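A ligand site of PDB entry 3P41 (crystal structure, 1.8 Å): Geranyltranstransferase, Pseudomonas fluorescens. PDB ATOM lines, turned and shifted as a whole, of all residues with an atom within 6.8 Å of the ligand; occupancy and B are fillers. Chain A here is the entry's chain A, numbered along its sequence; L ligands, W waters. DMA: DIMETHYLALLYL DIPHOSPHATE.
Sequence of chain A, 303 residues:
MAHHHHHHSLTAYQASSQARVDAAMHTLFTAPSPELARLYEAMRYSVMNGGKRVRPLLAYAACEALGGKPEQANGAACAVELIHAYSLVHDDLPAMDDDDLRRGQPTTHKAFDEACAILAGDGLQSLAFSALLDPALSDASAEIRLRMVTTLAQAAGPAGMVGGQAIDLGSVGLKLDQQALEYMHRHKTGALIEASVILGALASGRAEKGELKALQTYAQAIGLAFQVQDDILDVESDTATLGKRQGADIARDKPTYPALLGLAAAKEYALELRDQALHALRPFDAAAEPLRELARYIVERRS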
ATOM      1  N   ASN A  49      17.863 -34.407  32.563  1.00  0.00           N
ATOM      2  CA  ASN A  49      16.853 -33.752  33.383  1.00  0.00           C
ATOM      3  C   ASN A  49      15.433 -33.954  32.854  1.00  0.00           C
ATOM      4  O   ASN A  49      14.468 -33.527  33.479  1.00  0.00           O
ATOM      5  CB  ASN A  49      17.141 -32.243  33.499  1.00  0.00           C
ATOM      6  CG  ASN A  49      17.362 -31.580  32.140  1.00  0.00           C
ATOM      7  OD1 ASN A  49      16.924 -32.092  31.092  1.00  0.00           O
ATOM      8  ND2 ASN A  49      18.031 -30.423  32.137  1.00  0.00           N
ATOM      9  N   GLY A  50      15.321 -34.598  31.690  1.00  0.00           N
ATOM     10  CA  GLY A  50      14.033 -34.903  31.086  1.00  0.00           C
ATOM     11  C   GLY A  50      13.553 -33.867  30.075  1.00  0.00           C
ATOM     12  O   GLY A  50      12.430 -33.979  29.577  1.00  0.00           O
ATOM     13  N   GLY A  51      14.390 -32.877  29.768  1.00  0.00           N
ATOM     14  CA  GLY A  51      14.002 -31.811  28.833  1.00  0.00           C
ATOM     15  C   GLY A  51      13.910 -32.228  27.374  1.00  0.00           C
ATOM     16  O   GLY A  51      14.426 -33.268  26.961  1.00  0.00           O
ATOM     17  N   LYS A  52      13.284 -31.401  26.547  1.00  0.00           N
ATOM     18  CA  LYS A  52      13.107 -31.735  25.137  1.00  0.00           C
ATOM     19  C   LYS A  52      14.234 -31.203  24.239  1.00  0.00           C
ATOM     20  O   LYS A  52      14.129 -31.273  23.019  1.00  0.00           O
ATOM     21  CB  LYS A  52      11.743 -31.206  24.664  1.00  0.00           C
ATOM     22  CG  LYS A  52      10.579 -31.731  25.486  1.00  0.00           C
ATOM     23  CD  LYS A  52      10.375 -33.227  25.267  1.00  0.00           C
ATOM     24  CE  LYS A  52      10.153 -33.524  23.781  1.00  0.00           C
ATOM     25  NZ  LYS A  52       9.543 -34.872  23.515  1.00  0.00           N
ATOM     26  N   ARG A  53      15.314 -30.683  24.832  1.00  0.00           N
ATOM     27  CA  ARG A  53      16.435 -30.083  24.093  1.00  0.00           C
ATOM     28  C   ARG A  53      15.992 -29.060  23.063  1.00  0.00           C
ATOM     29  O   ARG A  53      16.440 -29.114  21.915  1.00  0.00           O
ATOM     30  CB  ARG A  53      17.242 -31.144  23.347  1.00  0.00           C
ATOM     31  CG  ARG A  53      17.572 -32.399  24.156  1.00  0.00           C
ATOM     32  CD  ARG A  53      18.379 -32.062  25.369  1.00  0.00           C
ATOM     33  NE  ARG A  53      18.822 -33.314  25.989  1.00  0.00           N
ATOM     34  CZ  ARG A  53      19.128 -33.455  27.271  1.00  0.00           C
ATOM     35  NH1 ARG A  53      19.050 -32.420  28.102  1.00  0.00           N
ATOM     36  NH2 ARG A  53      19.523 -34.649  27.732  1.00  0.00           N
ATOM     37  N   VAL A  54      15.082 -28.182  23.446  1.00  0.00           N
ATOM     38  CA  VAL A  54      14.535 -27.239  22.482  1.00  0.00           C
ATOM     39  C   VAL A  54      15.586 -26.234  22.048  1.00  0.00           C
ATOM     40  O   VAL A  54      15.543 -25.721  20.944  1.00  0.00           O
ATOM     41  CB  VAL A  54      13.347 -26.488  23.067  1.00  0.00           C
ATOM     42  CG1 VAL A  54      12.799 -25.550  22.007  1.00  0.00           C
ATOM     43  CG2 VAL A  54      12.275 -27.463  23.530  1.00  0.00           C
ATOM     44  N   ARG A  55      16.585 -25.996  22.896  1.00  0.00           N
ATOM     45  CA  ARG A  55      17.570 -24.975  22.528  1.00  0.00           C
ATOM     46  C   ARG A  55      18.515 -25.499  21.445  1.00  0.00           C
ATOM     47  O   ARG A  55      18.763 -24.819  20.453  1.00  0.00           O
ATOM     48  CB  ARG A  55      18.294 -24.409  23.765  1.00  0.00           C
ATOM     49  CG  ARG A  55      17.371 -23.455  24.573  1.00  0.00           C
ATOM     50  CD  ARG A  55      17.849 -23.181  25.987  1.00  0.00           C
ATOM     51  NE  ARG A  55      16.822 -22.477  26.766  1.00  0.00           N
ATOM     52  CZ  ARG A  55      15.728 -23.043  27.273  1.00  0.00           C
ATOM     53  NH1 ARG A  55      15.472 -24.338  27.084  1.00  0.00           N
ATOM     54  NH2 ARG A  55      14.843 -22.300  27.954  1.00  0.00           N
ATOM     55  N   PRO A  56      18.992 -26.736  21.615  1.00  0.00           N
ATOM     56  CA  PRO A  56      19.667 -27.476  20.539  1.00  0.00           C
ATOM     57  C   PRO A  56      18.807 -27.555  19.284  1.00  0.00           C
ATOM     58  O   PRO A  56      19.281 -27.285  18.187  1.00  0.00           O
ATOM     59  CB  PRO A  56      19.908 -28.867  21.157  1.00  0.00           C
ATOM     60  CG  PRO A  56      20.053 -28.583  22.640  1.00  0.00           C
ATOM     61  CD  PRO A  56      18.960 -27.468  22.891  1.00  0.00           C
ATOM     62  N   LEU A  58      16.660 -25.465  18.269  1.00  0.00           N
ATOM     63  CA  LEU A  58      16.814 -24.135  17.689  1.00  0.00           C
ATOM     64  C   LEU A  58      18.150 -23.894  16.967  1.00  0.00           C
ATOM     65  O   LEU A  58      18.135 -23.396  15.864  1.00  0.00           O
ATOM     66  CB  LEU A  58      16.557 -23.057  18.754  1.00  0.00           C
ATOM     67  CG  LEU A  58      15.073 -22.867  19.118  1.00  0.00           C
ATOM     68  CD1 LEU A  58      15.042 -22.190  20.442  1.00  0.00           C
ATOM     69  CD2 LEU A  58      14.260 -22.086  18.014  1.00  0.00           C
ATOM     70  N   GLU A  81      22.586 -26.013  25.593  1.00  0.00           N
ATOM     71  CA  GLU A  81      21.994 -26.951  26.512  1.00  0.00           C
ATOM     72  C   GLU A  81      22.746 -27.040  27.851  1.00  0.00           C
ATOM     73  O   GLU A  81      22.154 -27.270  28.907  1.00  0.00           O
ATOM     74  CB  GLU A  81      21.797 -28.322  25.845  1.00  0.00           C
ATOM     75  CG  GLU A  81      20.961 -29.314  26.649  1.00  0.00           C
ATOM     76  CD  GLU A  81      19.469 -28.941  26.767  1.00  0.00           C
ATOM     77  OE1 GLU A  81      19.030 -28.033  26.023  1.00  0.00           O
ATOM     78  OE2 GLU A  81      18.754 -29.596  27.555  1.00  0.00           O
ATOM     79  N   HIS A  84      21.760 -23.991  29.741  1.00  0.00           N
ATOM     80  CA  HIS A  84      20.417 -24.242  30.260  1.00  0.00           C
ATOM     81  C   HIS A  84      20.414 -25.204  31.467  1.00  0.00           C
ATOM     82  O   HIS A  84      19.829 -24.933  32.522  1.00  0.00           O
ATOM     83  CB  HIS A  84      19.515 -24.702  29.097  1.00  0.00           C
ATOM     84  CG  HIS A  84      18.132 -25.091  29.510  1.00  0.00           C
ATOM     85  ND1 HIS A  84      17.245 -24.195  30.066  1.00  0.00           N
ATOM     86  CD2 HIS A  84      17.476 -26.281  29.440  1.00  0.00           C
ATOM     87  CE1 HIS A  84      16.118 -24.818  30.347  1.00  0.00           C
ATOM     88  NE2 HIS A  84      16.221 -26.079  29.962  1.00  0.00           N
ATOM     89  N   LEU A  88      19.288 -24.416  35.675  1.00  0.00           N
ATOM     90  CA  LEU A  88      18.244 -25.129  36.372  1.00  0.00           C
ATOM     91  C   LEU A  88      18.786 -25.700  37.677  1.00  0.00           C
ATOM     92  O   LEU A  88      18.139 -25.654  38.717  1.00  0.00           O
ATOM     93  CB  LEU A  88      17.687 -26.258  35.486  1.00  0.00           C
ATOM     94  CG  LEU A  88      17.065 -25.846  34.149  1.00  0.00           C
ATOM     95  CD1 LEU A  88      16.634 -27.106  33.401  1.00  0.00           C
ATOM     96  CD2 LEU A  88      15.901 -24.896  34.363  1.00  0.00           C
ATOM     97  N   ARG A 103      10.478 -31.978  36.871  1.00  0.00           N
ATOM     98  CA  ARG A 103       9.952 -32.876  35.875  1.00  0.00           C
ATOM     99  C   ARG A 103       9.807 -34.273  36.435  1.00  0.00           C
ATOM    100  O   ARG A 103      10.099 -35.213  35.786  1.00  0.00           O
ATOM    101  CB  ARG A 103      10.787 -32.851  34.609  1.00  0.00           C
ATOM    102  CG  ARG A 103      10.500 -31.618  33.752  1.00  0.00           C
ATOM    103  CD  ARG A 103      11.089 -31.739  32.379  1.00  0.00           C
ATOM    104  NE  ARG A 103      10.535 -30.748  31.462  1.00  0.00           N
ATOM    105  CZ  ARG A 103      11.239 -29.751  30.959  1.00  0.00           C
ATOM    106  NH1 ARG A 103      10.681 -28.921  30.115  1.00  0.00           N
ATOM    107  NH2 ARG A 103      12.352 -29.382  31.544  1.00  0.00           N
ATOM    108  N   THR A 189      14.806 -15.890  30.064  1.00  0.00           N
ATOM    109  CA  THR A 189      14.748 -16.929  29.030  1.00  0.00           C
ATOM    110  C   THR A 189      14.974 -16.413  27.590  1.00  0.00           C
ATOM    111  O   THR A 189      15.471 -17.143  26.759  1.00  0.00           O
ATOM    112  CB  THR A 189      13.420 -17.700  29.085  1.00  0.00           C
ATOM    113  OG1 THR A 189      12.326 -16.782  28.970  1.00  0.00           O
ATOM    114  CG2 THR A 189      13.295 -18.516  30.367  1.00  0.00           C
ATOM    115  N   ILE A 193      17.470 -18.123  24.349  1.00  0.00           N
ATOM    116  CA  ILE A 193      16.760 -18.538  23.152  1.00  0.00           C
ATOM    117  C   ILE A 193      17.311 -17.850  21.895  1.00  0.00           C
ATOM    118  O   ILE A 193      17.609 -18.517  20.900  1.00  0.00           O
ATOM    119  CB  ILE A 193      15.228 -18.353  23.334  1.00  0.00           C
ATOM    120  CG1 ILE A 193      14.723 -19.395  24.351  1.00  0.00           C
ATOM    121  CG2 ILE A 193      14.501 -18.435  21.981  1.00  0.00           C
ATOM    122  CD1 ILE A 193      13.288 -19.142  24.824  1.00  0.00           C
ATOM    123  N   SER A 196      20.589 -19.270  21.052  1.00  0.00           N
ATOM    124  CA  SER A 196      20.437 -20.551  20.387  1.00  0.00           C
ATOM    125  C   SER A 196      20.366 -20.405  18.857  1.00  0.00           C
ATOM    126  O   SER A 196      21.146 -21.003  18.115  1.00  0.00           O
ATOM    127  CB  SER A 196      19.248 -21.334  20.943  1.00  0.00           C
ATOM    128  OG  SER A 196      19.406 -21.617  22.322  1.00  0.00           O
ATOM    129  N   ILE A 222       9.251 -15.899  19.721  1.00  0.00           N
ATOM    130  CA  ILE A 222       8.907 -17.182  20.327  1.00  0.00           C
ATOM    131  C   ILE A 222       9.239 -17.255  21.808  1.00  0.00           C
ATOM    132  O   ILE A 222       8.558 -17.974  22.549  1.00  0.00           O
ATOM    133  CB  ILE A 222       9.502 -18.425  19.578  1.00  0.00           C
ATOM    134  CG1 ILE A 222      11.037 -18.462  19.694  1.00  0.00           C
ATOM    135  CG2 ILE A 222       8.986 -18.495  18.132  1.00  0.00           C
ATOM    136  CD1 ILE A 222      11.663 -19.867  19.372  1.00  0.00           C
ATOM    137  N   GLY A 223      10.278 -16.532  22.229  1.00  0.00           N
ATOM    138  CA  GLY A 223      10.690 -16.547  23.646  1.00  0.00           C
ATOM    139  C   GLY A 223       9.577 -15.997  24.529  1.00  0.00           C
ATOM    140  O   GLY A 223       9.277 -16.541  25.584  1.00  0.00           O
ATOM    141  N   PHE A 226       6.285 -18.287  24.345  1.00  0.00           N
ATOM    142  CA  PHE A 226       6.361 -19.366  25.296  1.00  0.00           C
ATOM    143  C   PHE A 226       5.908 -18.986  26.725  1.00  0.00           C
ATOM    144  O   PHE A 226       5.239 -19.769  27.414  1.00  0.00           O
ATOM    145  CB  PHE A 226       7.807 -19.879  25.352  1.00  0.00           C
ATOM    146  CG  PHE A 226       8.015 -20.916  26.385  1.00  0.00           C
ATOM    147  CD1 PHE A 226       8.716 -20.620  27.543  1.00  0.00           C
ATOM    148  CD2 PHE A 226       7.460 -22.171  26.220  1.00  0.00           C
ATOM    149  CE1 PHE A 226       8.897 -21.592  28.517  1.00  0.00           C
ATOM    150  CE2 PHE A 226       7.636 -23.152  27.195  1.00  0.00           C
ATOM    151  CZ  PHE A 226       8.352 -22.855  28.346  1.00  0.00           C
ATOM    152  N   ASP A 230       2.726 -20.276  28.667  1.00  0.00           N
ATOM    153  CA  ASP A 230       2.919 -20.963  29.949  1.00  0.00           C
ATOM    154  C   ASP A 230       1.870 -20.484  30.967  1.00  0.00           C
ATOM    155  O   ASP A 230       1.201 -21.298  31.613  1.00  0.00           O
ATOM    156  CB  ASP A 230       4.297 -20.718  30.518  1.00  0.00           C
ATOM    157  CG  ASP A 230       5.192 -21.926  30.401  1.00  0.00           C
ATOM    158  OD1 ASP A 230       4.854 -22.864  29.656  1.00  0.00           O
ATOM    159  OD2 ASP A 230       6.249 -21.918  31.079  1.00  0.00           O
ATOM    160  N   LEU A 294       7.759 -25.004  15.152  1.00  0.00           N
ATOM    161  CA  LEU A 294       7.932 -24.768  16.592  1.00  0.00           C
ATOM    162  C   LEU A 294       7.105 -23.538  17.042  1.00  0.00           C
ATOM    163  O   LEU A 294       6.452 -23.546  18.087  1.00  0.00           O
ATOM    164  CB  LEU A 294       9.386 -24.494  16.922  1.00  0.00           C
ATOM    165  CG  LEU A 294       9.777 -24.297  18.395  1.00  0.00           C
ATOM    166  CD1 LEU A 294       9.614 -25.541  19.225  1.00  0.00           C
ATOM    167  CD2 LEU A 294      11.227 -23.794  18.434  1.00  0.00           C
ATOM    168  N   ILE A 298       4.257 -23.873  20.056  1.00  0.00           N
ATOM    169  CA  ILE A 298       4.397 -23.200  21.336  1.00  0.00           C
ATOM    170  C   ILE A 298       3.076 -22.584  21.783  1.00  0.00           C
ATOM    171  O   ILE A 298       2.740 -22.638  22.960  1.00  0.00           O
ATOM    172  CB  ILE A 298       5.524 -22.154  21.241  1.00  0.00           C
ATOM    173  CG1 ILE A 298       6.883 -22.889  21.348  1.00  0.00           C
ATOM    174  CG2 ILE A 298       5.386 -21.083  22.326  1.00  0.00           C
ATOM    175  CD1 ILE A 298       8.076 -21.975  21.128  1.00  0.00           C
HETATM  176  C1  DMA L   1      11.808 -24.058  26.008  1.00  0.00           C
HETATM  177  O1  DMA L   1      11.095 -24.664  27.061  1.00  0.00           O
HETATM  178  C2  DMA L   1      10.936 -23.181  25.172  1.00  0.00           C
HETATM  179  C3  DMA L   1      11.574 -22.498  24.228  1.00  0.00           C
HETATM  180  C4  DMA L   1      13.063 -22.646  24.110  1.00  0.00           C
HETATM  181  C5  DMA L   1      10.827 -21.581  23.311  1.00  0.00           C
HETATM  182  PA  DMA L   1      12.040 -25.383  28.154  1.00  0.00           P
HETATM  183  O1A DMA L   1      11.179 -26.106  29.188  1.00  0.00           O
HETATM  184  O2A DMA L   1      12.985 -24.321  28.646  1.00  0.00           O
HETATM  185  O3A DMA L   1      12.847 -26.394  27.176  1.00  0.00           O
HETATM  186  PB  DMA L   1      13.494 -27.826  27.536  1.00  0.00           P
HETATM  187  O1B DMA L   1      12.341 -28.821  27.436  1.00  0.00           O
HETATM  188  O2B DMA L   1      13.993 -27.652  28.977  1.00  0.00           O
HETATM  189  O3B DMA L   1      14.555 -28.020  26.438  1.00  0.00           O
HETATM  190  O   HOH W   1      16.292 -29.663  27.351  1.00  0.00           O
HETATM  191  O   HOH W   2      12.590 -22.262  30.179  1.00  0.00           O
HETATM  192  O   HOH W   3      15.905 -29.125  30.533  1.00  0.00           O
HETATM  193  O   HOH W   4      16.893 -26.792  25.793  1.00  0.00           O
HETATM  194  O   HOH W   5      12.828 -25.649  31.693  1.00  0.00           O
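Gly 51 touches the ligand (CA to O1B, 3.7 Å). Ile 193 touches the ligand. Phe 226 touches the ligand. Ile 298 touches the ligand. Hydrophobic or aromatic side chains that line the ligand: Val 54, His 84, Ile 193, Phe 226 and Ile 298. Ten residues have an atom within 4 Å of the ligand: Gly 51, Lys 52, Arg 53, Val 54, Arg 55, His 84, Arg 103, Ile 193, Phe 226 and Ile 298. The nearest printed residue that does not touch the ligand is Leu 58 (4.2 Å).
Water W1 lies within hydrogen-bond range of the side-chain carboxylate (OE2) of Glu 81 (2.5 Å), an oxygen (O3B) of the ligand (2.6 Å) and the backbone NH (N) of Arg 53 (2.9 Å). Water W2 bridges O2A of the ligand (2.6 Å) and NH2 of Arg 55 (3.2 Å). Water W4 lies within hydrogen-bond range of the side-chain carboxylate of Glu 81 (2.5 Å), an oxygen (O3B) of the ligand (2.7 Å), the backbone NH of Arg 55 (3.0 Å) and the backbone NH of Val 54 (3.3 Å). Water W3 lies within hydrogen-bond range of O2B of the ligand (2.9 Å), ND2 of Asn 49 (3.0 Å) and NE2 of His 84 (3.1 Å).
NH1 of Arg 53 lies within salt-bridge range of OE2 of Glu 81 (2.9 Å). The guanidinium group of Arg 55 lies close to a ring nitrogen (NE2) of His 84 (3.4 Å). The backbone NH of Gly 51 is in hydrogen-bond range of the side-chain amide oxygen of Asn 49 (3.0 Å).
An oxygen (O3B) of the ligand is in hydrogen-bond range of the backbone NH of Arg 53 (3.2 Å). A ring nitrogen (NE2) of His 84 lies within hydrogen-bond range of an oxygen (O2B) of the ligand (2.9 Å). O1B of the ligand lies within hydrogen-bond range of N of Lys 52 (2.9 Å). O3B of the ligand is in hydrogen-bond range of N of Val 54, 3.0 Å away. The guanidinium group (NH1) of Arg 103 lies within salt-bridge range of an oxygen (O1A) of the ligand, at 3.0 Å. The guanidinium group of Arg 55 lies within salt-bridge range of an oxygen (O2A) of the ligand, at 2.8 Å.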
